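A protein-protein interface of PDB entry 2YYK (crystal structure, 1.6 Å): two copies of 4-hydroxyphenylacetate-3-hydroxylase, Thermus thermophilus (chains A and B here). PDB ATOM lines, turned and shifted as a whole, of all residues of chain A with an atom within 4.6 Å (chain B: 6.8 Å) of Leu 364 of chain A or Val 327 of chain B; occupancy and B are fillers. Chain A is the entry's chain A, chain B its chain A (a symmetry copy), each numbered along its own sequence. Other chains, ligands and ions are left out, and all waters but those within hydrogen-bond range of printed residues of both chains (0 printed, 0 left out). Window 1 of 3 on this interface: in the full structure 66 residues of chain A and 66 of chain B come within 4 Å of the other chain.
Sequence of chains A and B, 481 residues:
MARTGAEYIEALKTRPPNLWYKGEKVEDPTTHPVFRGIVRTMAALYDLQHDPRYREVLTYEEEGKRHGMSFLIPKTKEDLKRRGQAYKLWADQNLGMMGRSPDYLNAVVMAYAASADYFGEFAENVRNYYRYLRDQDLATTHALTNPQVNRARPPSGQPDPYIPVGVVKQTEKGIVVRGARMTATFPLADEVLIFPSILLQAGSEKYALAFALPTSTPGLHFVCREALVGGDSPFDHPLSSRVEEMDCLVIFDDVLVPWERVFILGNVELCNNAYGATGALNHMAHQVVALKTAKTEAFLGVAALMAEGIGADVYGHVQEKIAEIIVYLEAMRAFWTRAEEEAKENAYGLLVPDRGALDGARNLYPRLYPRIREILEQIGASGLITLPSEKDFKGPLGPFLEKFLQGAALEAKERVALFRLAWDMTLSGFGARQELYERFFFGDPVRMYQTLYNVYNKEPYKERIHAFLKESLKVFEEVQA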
ATOM      1  N   PHE A 335      23.561 -16.808  -0.857  1.00  0.00           N
ATOM      2  CA  PHE A 335      23.929 -16.636  -2.261  1.00  0.00           C
ATOM      3  C   PHE A 335      24.744 -15.360  -2.433  1.00  0.00           C
ATOM      4  O   PHE A 335      25.725 -15.332  -3.166  1.00  0.00           O
ATOM      5  CB  PHE A 335      22.685 -16.530  -3.151  1.00  0.00           C
ATOM      6  CG  PHE A 335      22.025 -17.848  -3.460  1.00  0.00           C
ATOM      7  CD1 PHE A 335      22.763 -18.918  -3.965  1.00  0.00           C
ATOM      8  CD2 PHE A 335      20.648 -17.990  -3.317  1.00  0.00           C
ATOM      9  CE1 PHE A 335      22.134 -20.110  -4.330  1.00  0.00           C
ATOM     10  CE2 PHE A 335      20.007 -19.172  -3.678  1.00  0.00           C
ATOM     11  CZ  PHE A 335      20.754 -20.235  -4.187  1.00  0.00           C
ATOM     12  N   GLY A 360      21.925 -19.286  -8.954  1.00  0.00           N
ATOM     13  CA  GLY A 360      21.083 -19.950  -7.971  1.00  0.00           C
ATOM     14  C   GLY A 360      20.067 -18.965  -7.411  1.00  0.00           C
ATOM     15  O   GLY A 360      18.872 -19.250  -7.347  1.00  0.00           O
ATOM     16  N   ALA A 361      20.538 -17.783  -7.023  1.00  0.00           N
ATOM     17  CA  ALA A 361      19.656 -16.769  -6.460  1.00  0.00           C
ATOM     18  C   ALA A 361      18.577 -16.282  -7.417  1.00  0.00           C
ATOM     19  O   ALA A 361      17.409 -16.196  -7.041  1.00  0.00           O
ATOM     20  CB  ALA A 361      20.477 -15.573  -5.969  1.00  0.00           C
ATOM     21  N   ARG A 362      18.963 -15.957  -8.649  1.00  0.00           N
ATOM     22  CA  ARG A 362      17.990 -15.431  -9.597  1.00  0.00           C
ATOM     23  C   ARG A 362      17.049 -16.471 -10.182  1.00  0.00           C
ATOM     24  O   ARG A 362      16.017 -16.123 -10.750  1.00  0.00           O
ATOM     25  CB  ARG A 362      18.693 -14.629 -10.701  1.00  0.00           C
ATOM     26  CG  ARG A 362      19.511 -15.436 -11.684  1.00  0.00           C
ATOM     27  CD  ARG A 362      20.525 -14.533 -12.375  1.00  0.00           C
ATOM     28  NE  ARG A 362      21.212 -15.235 -13.453  1.00  0.00           N
ATOM     29  CZ  ARG A 362      20.865 -15.157 -14.732  1.00  0.00           C
ATOM     30  NH1 ARG A 362      21.542 -15.842 -15.644  1.00  0.00           N
ATOM     31  NH2 ARG A 362      19.850 -14.381 -15.103  1.00  0.00           N
ATOM     32  N   ASN A 363      17.391 -17.746 -10.039  1.00  0.00           N
ATOM     33  CA  ASN A 363      16.503 -18.793 -10.530  1.00  0.00           C
ATOM     34  C   ASN A 363      15.652 -19.373  -9.409  1.00  0.00           C
ATOM     35  O   ASN A 363      14.648 -20.045  -9.664  1.00  0.00           O
ATOM     36  CB  ASN A 363      17.302 -19.886 -11.241  1.00  0.00           C
ATOM     37  CG  ASN A 363      17.645 -19.494 -12.660  1.00  0.00           C
ATOM     38  OD1 ASN A 363      16.751 -19.342 -13.494  1.00  0.00           O
ATOM     39  ND2 ASN A 363      18.931 -19.303 -12.940  1.00  0.00           N
ATOM     40  N   LEU A 364      16.036 -19.107  -8.164  1.00  0.00           N
ATOM     41  CA  LEU A 364      15.260 -19.603  -7.034  1.00  0.00           C
ATOM     42  C   LEU A 364      14.256 -18.563  -6.530  1.00  0.00           C
ATOM     43  O   LEU A 364      13.107 -18.897  -6.241  1.00  0.00           O
ATOM     44  CB  LEU A 364      16.175 -20.021  -5.875  1.00  0.00           C
ATOM     45  CG  LEU A 364      15.460 -20.648  -4.669  1.00  0.00           C
ATOM     46  CD1 LEU A 364      14.748 -21.934  -5.087  1.00  0.00           C
ATOM     47  CD2 LEU A 364      16.467 -20.947  -3.570  1.00  0.00           C
ATOM     48  N   TYR A 365      14.668 -17.301  -6.450  1.00  0.00           N
ATOM     49  CA  TYR A 365      13.760 -16.288  -5.923  1.00  0.00           C
ATOM     50  C   TYR A 365      12.429 -16.149  -6.652  1.00  0.00           C
ATOM     51  O   TYR A 365      11.411 -15.876  -6.021  1.00  0.00           O
ATOM     52  CB  TYR A 365      14.449 -14.921  -5.814  1.00  0.00           C
ATOM     53  CG  TYR A 365      13.786 -14.043  -4.776  1.00  0.00           C
ATOM     54  CD1 TYR A 365      12.953 -12.989  -5.153  1.00  0.00           C
ATOM     55  CD2 TYR A 365      13.938 -14.312  -3.416  1.00  0.00           C
ATOM     56  CE1 TYR A 365      12.283 -12.224  -4.193  1.00  0.00           C
ATOM     57  CE2 TYR A 365      13.271 -13.558  -2.448  1.00  0.00           C
ATOM     58  CZ  TYR A 365      12.445 -12.516  -2.846  1.00  0.00           C
ATOM     59  OH  TYR A 365      11.772 -11.763  -1.903  1.00  0.00           O
ATOM     60  N   PRO A 366      12.413 -16.309  -7.987  1.00  0.00           N
ATOM     61  CA  PRO A 366      11.121 -16.183  -8.677  1.00  0.00           C
ATOM     62  C   PRO A 366      10.122 -17.237  -8.193  1.00  0.00           C
ATOM     63  O   PRO A 366       8.912 -17.085  -8.369  1.00  0.00           O
ATOM     64  CB  PRO A 366      11.494 -16.362 -10.149  1.00  0.00           C
ATOM     65  CG  PRO A 366      12.875 -15.767 -10.213  1.00  0.00           C
ATOM     66  CD  PRO A 366      13.527 -16.321  -8.953  1.00  0.00           C
ATOM     67  N   ARG A 367      10.631 -18.311  -7.593  1.00  0.00           N
ATOM     68  CA  ARG A 367       9.776 -19.373  -7.063  1.00  0.00           C
ATOM     69  C   ARG A 367       9.452 -19.099  -5.596  1.00  0.00           C
ATOM     70  O   ARG A 367       8.354 -19.404  -5.122  1.00  0.00           O
ATOM     71  CB  ARG A 367      10.464 -20.736  -7.176  1.00  0.00           C
ATOM     72  CG  ARG A 367      10.748 -21.189  -8.596  1.00  0.00           C
ATOM     73  CD  ARG A 367      11.398 -22.559  -8.574  1.00  0.00           C
ATOM     74  NE  ARG A 367      10.535 -23.537  -7.921  1.00  0.00           N
ATOM     75  CZ  ARG A 367      10.972 -24.624  -7.295  1.00  0.00           C
ATOM     76  NH1 ARG A 367      10.107 -25.459  -6.733  1.00  0.00           N
ATOM     77  NH2 ARG A 367      12.273 -24.871  -7.217  1.00  0.00           N
ATOM     78  N   LEU A 368      10.409 -18.524  -4.874  1.00  0.00           N
ATOM     79  CA  LEU A 368      10.210 -18.215  -3.463  1.00  0.00           C
ATOM     80  C   LEU A 368       9.244 -17.059  -3.251  1.00  0.00           C
ATOM     81  O   LEU A 368       8.417 -17.100  -2.345  1.00  0.00           O
ATOM     82  CB  LEU A 368      11.536 -17.852  -2.789  1.00  0.00           C
ATOM     83  CG  LEU A 368      12.666 -18.874  -2.845  1.00  0.00           C
ATOM     84  CD1 LEU A 368      13.838 -18.344  -2.028  1.00  0.00           C
ATOM     85  CD2 LEU A 368      12.197 -20.216  -2.302  1.00  0.00           C
ATOM     86  N   TYR A 449      16.081 -21.559 -16.987  1.00  0.00           N
ATOM     87  CA  TYR A 449      16.522 -22.861 -16.507  1.00  0.00           C
ATOM     88  C   TYR A 449      17.244 -23.632 -17.613  1.00  0.00           C
ATOM     89  O   TYR A 449      18.217 -24.339 -17.350  1.00  0.00           O
ATOM     90  CB  TYR A 449      15.333 -23.657 -15.949  1.00  0.00           C
ATOM     91  CG  TYR A 449      15.085 -23.396 -14.472  1.00  0.00           C
ATOM     92  CD1 TYR A 449      14.770 -22.113 -14.009  1.00  0.00           C
ATOM     93  CD2 TYR A 449      15.201 -24.420 -13.532  1.00  0.00           C
ATOM     94  CE1 TYR A 449      14.582 -21.859 -12.647  1.00  0.00           C
ATOM     95  CE2 TYR A 449      15.017 -24.178 -12.168  1.00  0.00           C
ATOM     96  CZ  TYR A 449      14.710 -22.896 -11.732  1.00  0.00           C
ATOM     97  OH  TYR A 449      14.542 -22.657 -10.384  1.00  0.00           O
ATOM     98  N   LEU A 452      20.662 -22.185 -17.779  1.00  0.00           N
ATOM     99  CA  LEU A 452      21.486 -22.666 -16.675  1.00  0.00           C
ATOM    100  C   LEU A 452      21.995 -24.075 -16.969  1.00  0.00           C
ATOM    101  O   LEU A 452      23.162 -24.392 -16.728  1.00  0.00           O
ATOM    102  CB  LEU A 452      20.690 -22.661 -15.366  1.00  0.00           C
ATOM    103  CG  LEU A 452      21.418 -23.233 -14.144  1.00  0.00           C
ATOM    104  CD1 LEU A 452      22.749 -22.510 -13.944  1.00  0.00           C
ATOM    105  CD2 LEU A 452      20.536 -23.074 -12.903  1.00  0.00           C
ATOM    106  N   ILE B 322      17.085 -30.803 -14.361  1.00  0.00           N
ATOM    107  CA  ILE B 322      18.491 -30.892 -13.990  1.00  0.00           C
ATOM    108  C   ILE B 322      18.968 -29.523 -13.499  1.00  0.00           C
ATOM    109  O   ILE B 322      19.747 -29.433 -12.547  1.00  0.00           O
ATOM    110  CB  ILE B 322      19.342 -31.397 -15.177  1.00  0.00           C
ATOM    111  CG1 ILE B 322      18.942 -32.842 -15.493  1.00  0.00           C
ATOM    112  CG2 ILE B 322      20.823 -31.334 -14.841  1.00  0.00           C
ATOM    113  CD1 ILE B 322      19.635 -33.443 -16.704  1.00  0.00           C
ATOM    114  N   ALA B 323      18.488 -28.459 -14.135  1.00  0.00           N
ATOM    115  CA  ALA B 323      18.843 -27.106 -13.714  1.00  0.00           C
ATOM    116  C   ALA B 323      18.308 -26.851 -12.301  1.00  0.00           C
ATOM    117  O   ALA B 323      18.907 -26.099 -11.525  1.00  0.00           O
ATOM    118  CB  ALA B 323      18.267 -26.083 -14.695  1.00  0.00           C
ATOM    119  N   GLU B 324      17.175 -27.474 -11.972  1.00  0.00           N
ATOM    120  CA  GLU B 324      16.579 -27.322 -10.648  1.00  0.00           C
ATOM    121  C   GLU B 324      17.520 -27.945  -9.620  1.00  0.00           C
ATOM    122  O   GLU B 324      17.737 -27.386  -8.545  1.00  0.00           O
ATOM    123  CB  GLU B 324      15.209 -28.012 -10.580  1.00  0.00           C
ATOM    124  CG  GLU B 324      14.441 -27.691  -9.301  1.00  0.00           C
ATOM    125  CD  GLU B 324      13.043 -28.290  -9.284  1.00  0.00           C
ATOM    126  OE1 GLU B 324      12.483 -28.537 -10.375  1.00  0.00           O
ATOM    127  OE2 GLU B 324      12.497 -28.497  -8.179  1.00  0.00           O
ATOM    128  N   ILE B 325      18.090 -29.102  -9.958  1.00  0.00           N
ATOM    129  CA  ILE B 325      19.027 -29.751  -9.049  1.00  0.00           C
ATOM    130  C   ILE B 325      20.243 -28.836  -8.891  1.00  0.00           C
ATOM    131  O   ILE B 325      20.790 -28.706  -7.802  1.00  0.00           O
ATOM    132  CB  ILE B 325      19.490 -31.130  -9.578  1.00  0.00           C
ATOM    133  CG1 ILE B 325      18.319 -32.115  -9.551  1.00  0.00           C
ATOM    134  CG2 ILE B 325      20.642 -31.665  -8.717  1.00  0.00           C
ATOM    135  CD1 ILE B 325      18.665 -33.504 -10.080  1.00  0.00           C
ATOM    136  N   ILE B 326      20.658 -28.198  -9.983  1.00  0.00           N
ATOM    137  CA  ILE B 326      21.800 -27.287  -9.936  1.00  0.00           C
ATOM    138  C   ILE B 326      21.521 -26.110  -8.997  1.00  0.00           C
ATOM    139  O   ILE B 326      22.394 -25.703  -8.231  1.00  0.00           O
ATOM    140  CB  ILE B 326      22.153 -26.768 -11.352  1.00  0.00           C
ATOM    141  CG1 ILE B 326      22.729 -27.917 -12.185  1.00  0.00           C
ATOM    142  CG2 ILE B 326      23.159 -25.619 -11.262  1.00  0.00           C
ATOM    143  CD1 ILE B 326      22.830 -27.616 -13.679  1.00  0.00           C
ATOM    144  N   VAL B 327      20.305 -25.568  -9.047  1.00  0.00           N
ATOM    145  CA  VAL B 327      19.939 -24.459  -8.169  1.00  0.00           C
ATOM    146  C   VAL B 327      20.055 -24.899  -6.707  1.00  0.00           C
ATOM    147  O   VAL B 327      20.602 -24.173  -5.874  1.00  0.00           O
ATOM    148  CB  VAL B 327      18.492 -23.966  -8.457  1.00  0.00           C
ATOM    149  CG1 VAL B 327      18.051 -22.945  -7.403  1.00  0.00           C
ATOM    150  CG2 VAL B 327      18.436 -23.321  -9.838  1.00  0.00           C
ATOM    151  N   TYR B 328      19.559 -26.093  -6.397  1.00  0.00           N
ATOM    152  CA  TYR B 328      19.625 -26.603  -5.029  1.00  0.00           C
ATOM    153  C   TYR B 328      21.072 -26.850  -4.599  1.00  0.00           C
ATOM    154  O   TYR B 328      21.435 -26.579  -3.458  1.00  0.00           O
ATOM    155  CB  TYR B 328      18.797 -27.890  -4.895  1.00  0.00           C
ATOM    156  CG  TYR B 328      17.320 -27.711  -5.213  1.00  0.00           C
ATOM    157  CD1 TYR B 328      16.713 -26.456  -5.139  1.00  0.00           C
ATOM    158  CD2 TYR B 328      16.534 -28.801  -5.583  1.00  0.00           C
ATOM    159  CE1 TYR B 328      15.352 -26.295  -5.434  1.00  0.00           C
ATOM    160  CE2 TYR B 328      15.178 -28.650  -5.876  1.00  0.00           C
ATOM    161  CZ  TYR B 328      14.595 -27.399  -5.804  1.00  0.00           C
ATOM    162  OH  TYR B 328      13.255 -27.251  -6.111  1.00  0.00           O
ATOM    163  N   LEU B 329      21.897 -27.347  -5.516  1.00  0.00           N
ATOM    164  CA  LEU B 329      23.304 -27.596  -5.207  1.00  0.00           C
ATOM    165  C   LEU B 329      23.977 -26.274  -4.867  1.00  0.00           C
ATOM    166  O   LEU B 329      24.746 -26.185  -3.908  1.00  0.00           O
ATOM    167  CB  LEU B 329      24.021 -28.236  -6.404  1.00  0.00           C
ATOM    168  CG  LEU B 329      25.554 -28.313  -6.325  1.00  0.00           C
ATOM    169  CD1 LEU B 329      25.987 -29.064  -5.063  1.00  0.00           C
ATOM    170  CD2 LEU B 329      26.091 -29.004  -7.583  1.00  0.00           C
ATOM    171  N   GLU B 330      23.696 -25.247  -5.662  1.00  0.00           N
ATOM    172  CA  GLU B 330      24.289 -23.942  -5.409  1.00  0.00           C
ATOM    173  C   GLU B 330      23.775 -23.355  -4.088  1.00  0.00           C
ATOM    174  O   GLU B 330      24.524 -22.704  -3.360  1.00  0.00           O
ATOM    175  CB  GLU B 330      24.011 -22.999  -6.582  1.00  0.00           C
ATOM    176  CG  GLU B 330      24.805 -23.339  -7.857  1.00  0.00           C
ATOM    177  CD  GLU B 330      26.300 -23.132  -7.691  1.00  0.00           C
ATOM    178  OE1 GLU B 330      26.690 -22.227  -6.928  1.00  0.00           O
ATOM    179  OE2 GLU B 330      27.090 -23.857  -8.339  1.00  0.00           O
ATOM    180  N   ALA B 331      22.507 -23.598  -3.761  1.00  0.00           N
ATOM    181  CA  ALA B 331      21.961 -23.092  -2.503  1.00  0.00           C
ATOM    182  C   ALA B 331      22.732 -23.689  -1.326  1.00  0.00           C
ATOM    183  O   ALA B 331      23.105 -22.981  -0.384  1.00  0.00           O
ATOM    184  CB  ALA B 331      20.474 -23.443  -2.383  1.00  0.00           C
ATOM    185  N   MET B 332      22.969 -24.994  -1.383  1.00  0.00           N
ATOM    186  CA  MET B 332      23.684 -25.664  -0.305  1.00  0.00           C
ATOM    187  C   MET B 332      25.135 -25.193  -0.219  1.00  0.00           C
ATOM    188  O   MET B 332      25.664 -25.007   0.881  1.00  0.00           O
ATOM    189  CB  MET B 332      23.590 -27.184  -0.479  1.00  0.00           C
ATOM    190  CG  MET B 332      22.157 -27.714  -0.389  1.00  0.00           C
ATOM    191  SD  MET B 332      21.298 -27.228   1.135  1.00  0.00           S
ATOM    192  CE  MET B 332      21.961 -28.409   2.274  1.00  0.00           C
ATOM    193  N   LEU B 364      15.992 -26.335   5.072  1.00  0.00           N
ATOM    194  CA  LEU B 364      15.584 -26.326   3.673  1.00  0.00           C
ATOM    195  C   LEU B 364      15.833 -27.676   2.997  1.00  0.00           C
ATOM    196  O   LEU B 364      14.982 -28.164   2.252  1.00  0.00           O
ATOM    197  CB  LEU B 364      16.320 -25.229   2.890  1.00  0.00           C
ATOM    198  CG  LEU B 364      15.891 -25.072   1.423  1.00  0.00           C
ATOM    199  CD1 LEU B 364      14.414 -24.686   1.343  1.00  0.00           C
ATOM    200  CD2 LEU B 364      16.742 -24.009   0.748  1.00  0.00           C
ATOM    201  N   LEU B 368      14.024 -30.041   0.052  1.00  0.00           N
ATOM    202  CA  LEU B 368      14.631 -30.183  -1.266  1.00  0.00           C
ATOM    203  C   LEU B 368      14.872 -31.637  -1.643  1.00  0.00           C
ATOM    204  O   LEU B 368      14.655 -32.024  -2.788  1.00  0.00           O
ATOM    205  CB  LEU B 368      15.973 -29.449  -1.332  1.00  0.00           C
ATOM    206  CG  LEU B 368      15.984 -27.957  -1.016  1.00  0.00           C
ATOM    207  CD1 LEU B 368      17.394 -27.425  -1.245  1.00  0.00           C
ATOM    208  CD2 LEU B 368      14.984 -27.219  -1.894  1.00  0.00           C
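NH2 of Arg 367 of chain A is in salt-bridge range of OE2 of Glu 324 of chain B (3.8 Å). The side-chain hydroxyl of Tyr 328 of chain B sits at hydrogen-bond distance from the guanidinium group of Arg 367 of chain A, 2.8 Å away.
The side-chain carboxylate of Glu 324 of chain B sits at hydrogen-bond distance from the side-chain hydroxyl of Tyr 328 of chain B. The backbone carbonyl oxygen (O) of Asn 363 of chain A lies within hydrogen-bond range of the side-chain hydroxyl (OH) of Tyr 449 of chain A, at 2.7 Å.
CE1 of Phe 335 of chain A touches C of Glu 330 of chain B, at 3.6 Å. CA of Ala 331 of chain B touches CE1 of Phe 335 of chain A, 3.5 Å away. Gly 360 of chain A touches Val 327 of chain B. Asn 363 of chain A touches Val 327 of chain B (CB to CG2, 3.9 Å). CB of Leu 364 of chain A touches CG1 of Val 327 of chain B (3.8 Å). Tyr 449 of chain A touches Ala 323 of chain B (O to CB, 3.2 Å). Tyr 449 of chain A touches Glu 324 of chain B. Tyr 449 of chain A touches Val 327 of chain B (OH to CG2, 3.99 Å). Ala 323 of chain B touches Leu 452 of chain A (O to CD2, 3.7 Å). CD2 of Leu 452 of chain A touches CG2 of Val 327 of chain B, at 3.7 Å.
Leu 364 of chain A touches one residue of chain B. Of the printed residues of chain A, Val 327 of chain B touches Gly 360 (3.8 Å), Asn 363 (3.9 Å), Leu 364 (3.8 Å), Tyr 449 (3.99 Å) and Leu 452 (3.7 Å). Printed residues of chain B within 4 Å of Gly 360 of chain A: Val 327. Of the printed residues of chain A, Ala 323 of chain B touches Tyr 449 and Leu 452. Printed residues of chain A within 4 Å of Tyr 328 of chain B: Arg 367 (2.8 Å). Of the printed residues of chain B, Arg 367 of chain A touches Glu 324 (3.8 Å) and Tyr 328 (2.8 Å). Ile 325 of chain B touches none of the printed residues of chain A.
Hydrophobic or aromatic side chains of chain A within 4 Å of the printed part of chain B: Phe 335, Leu 364, Tyr 449 and Leu 452. Of the 13 printed residues of chain B, 6 touch a printed residue of chain A. Hydrophobic or aromatic side chains of chain B that line the printed part of chain A: Ala 323, Val 327, Tyr 328 and Ala 331. Among the printed residues, 12 pairs touch across the chains.
2 positions are printed for both chains. Of the 12 pairs that touch across the chains among the printed residues, none has its exchanged pair printed and touching as well.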
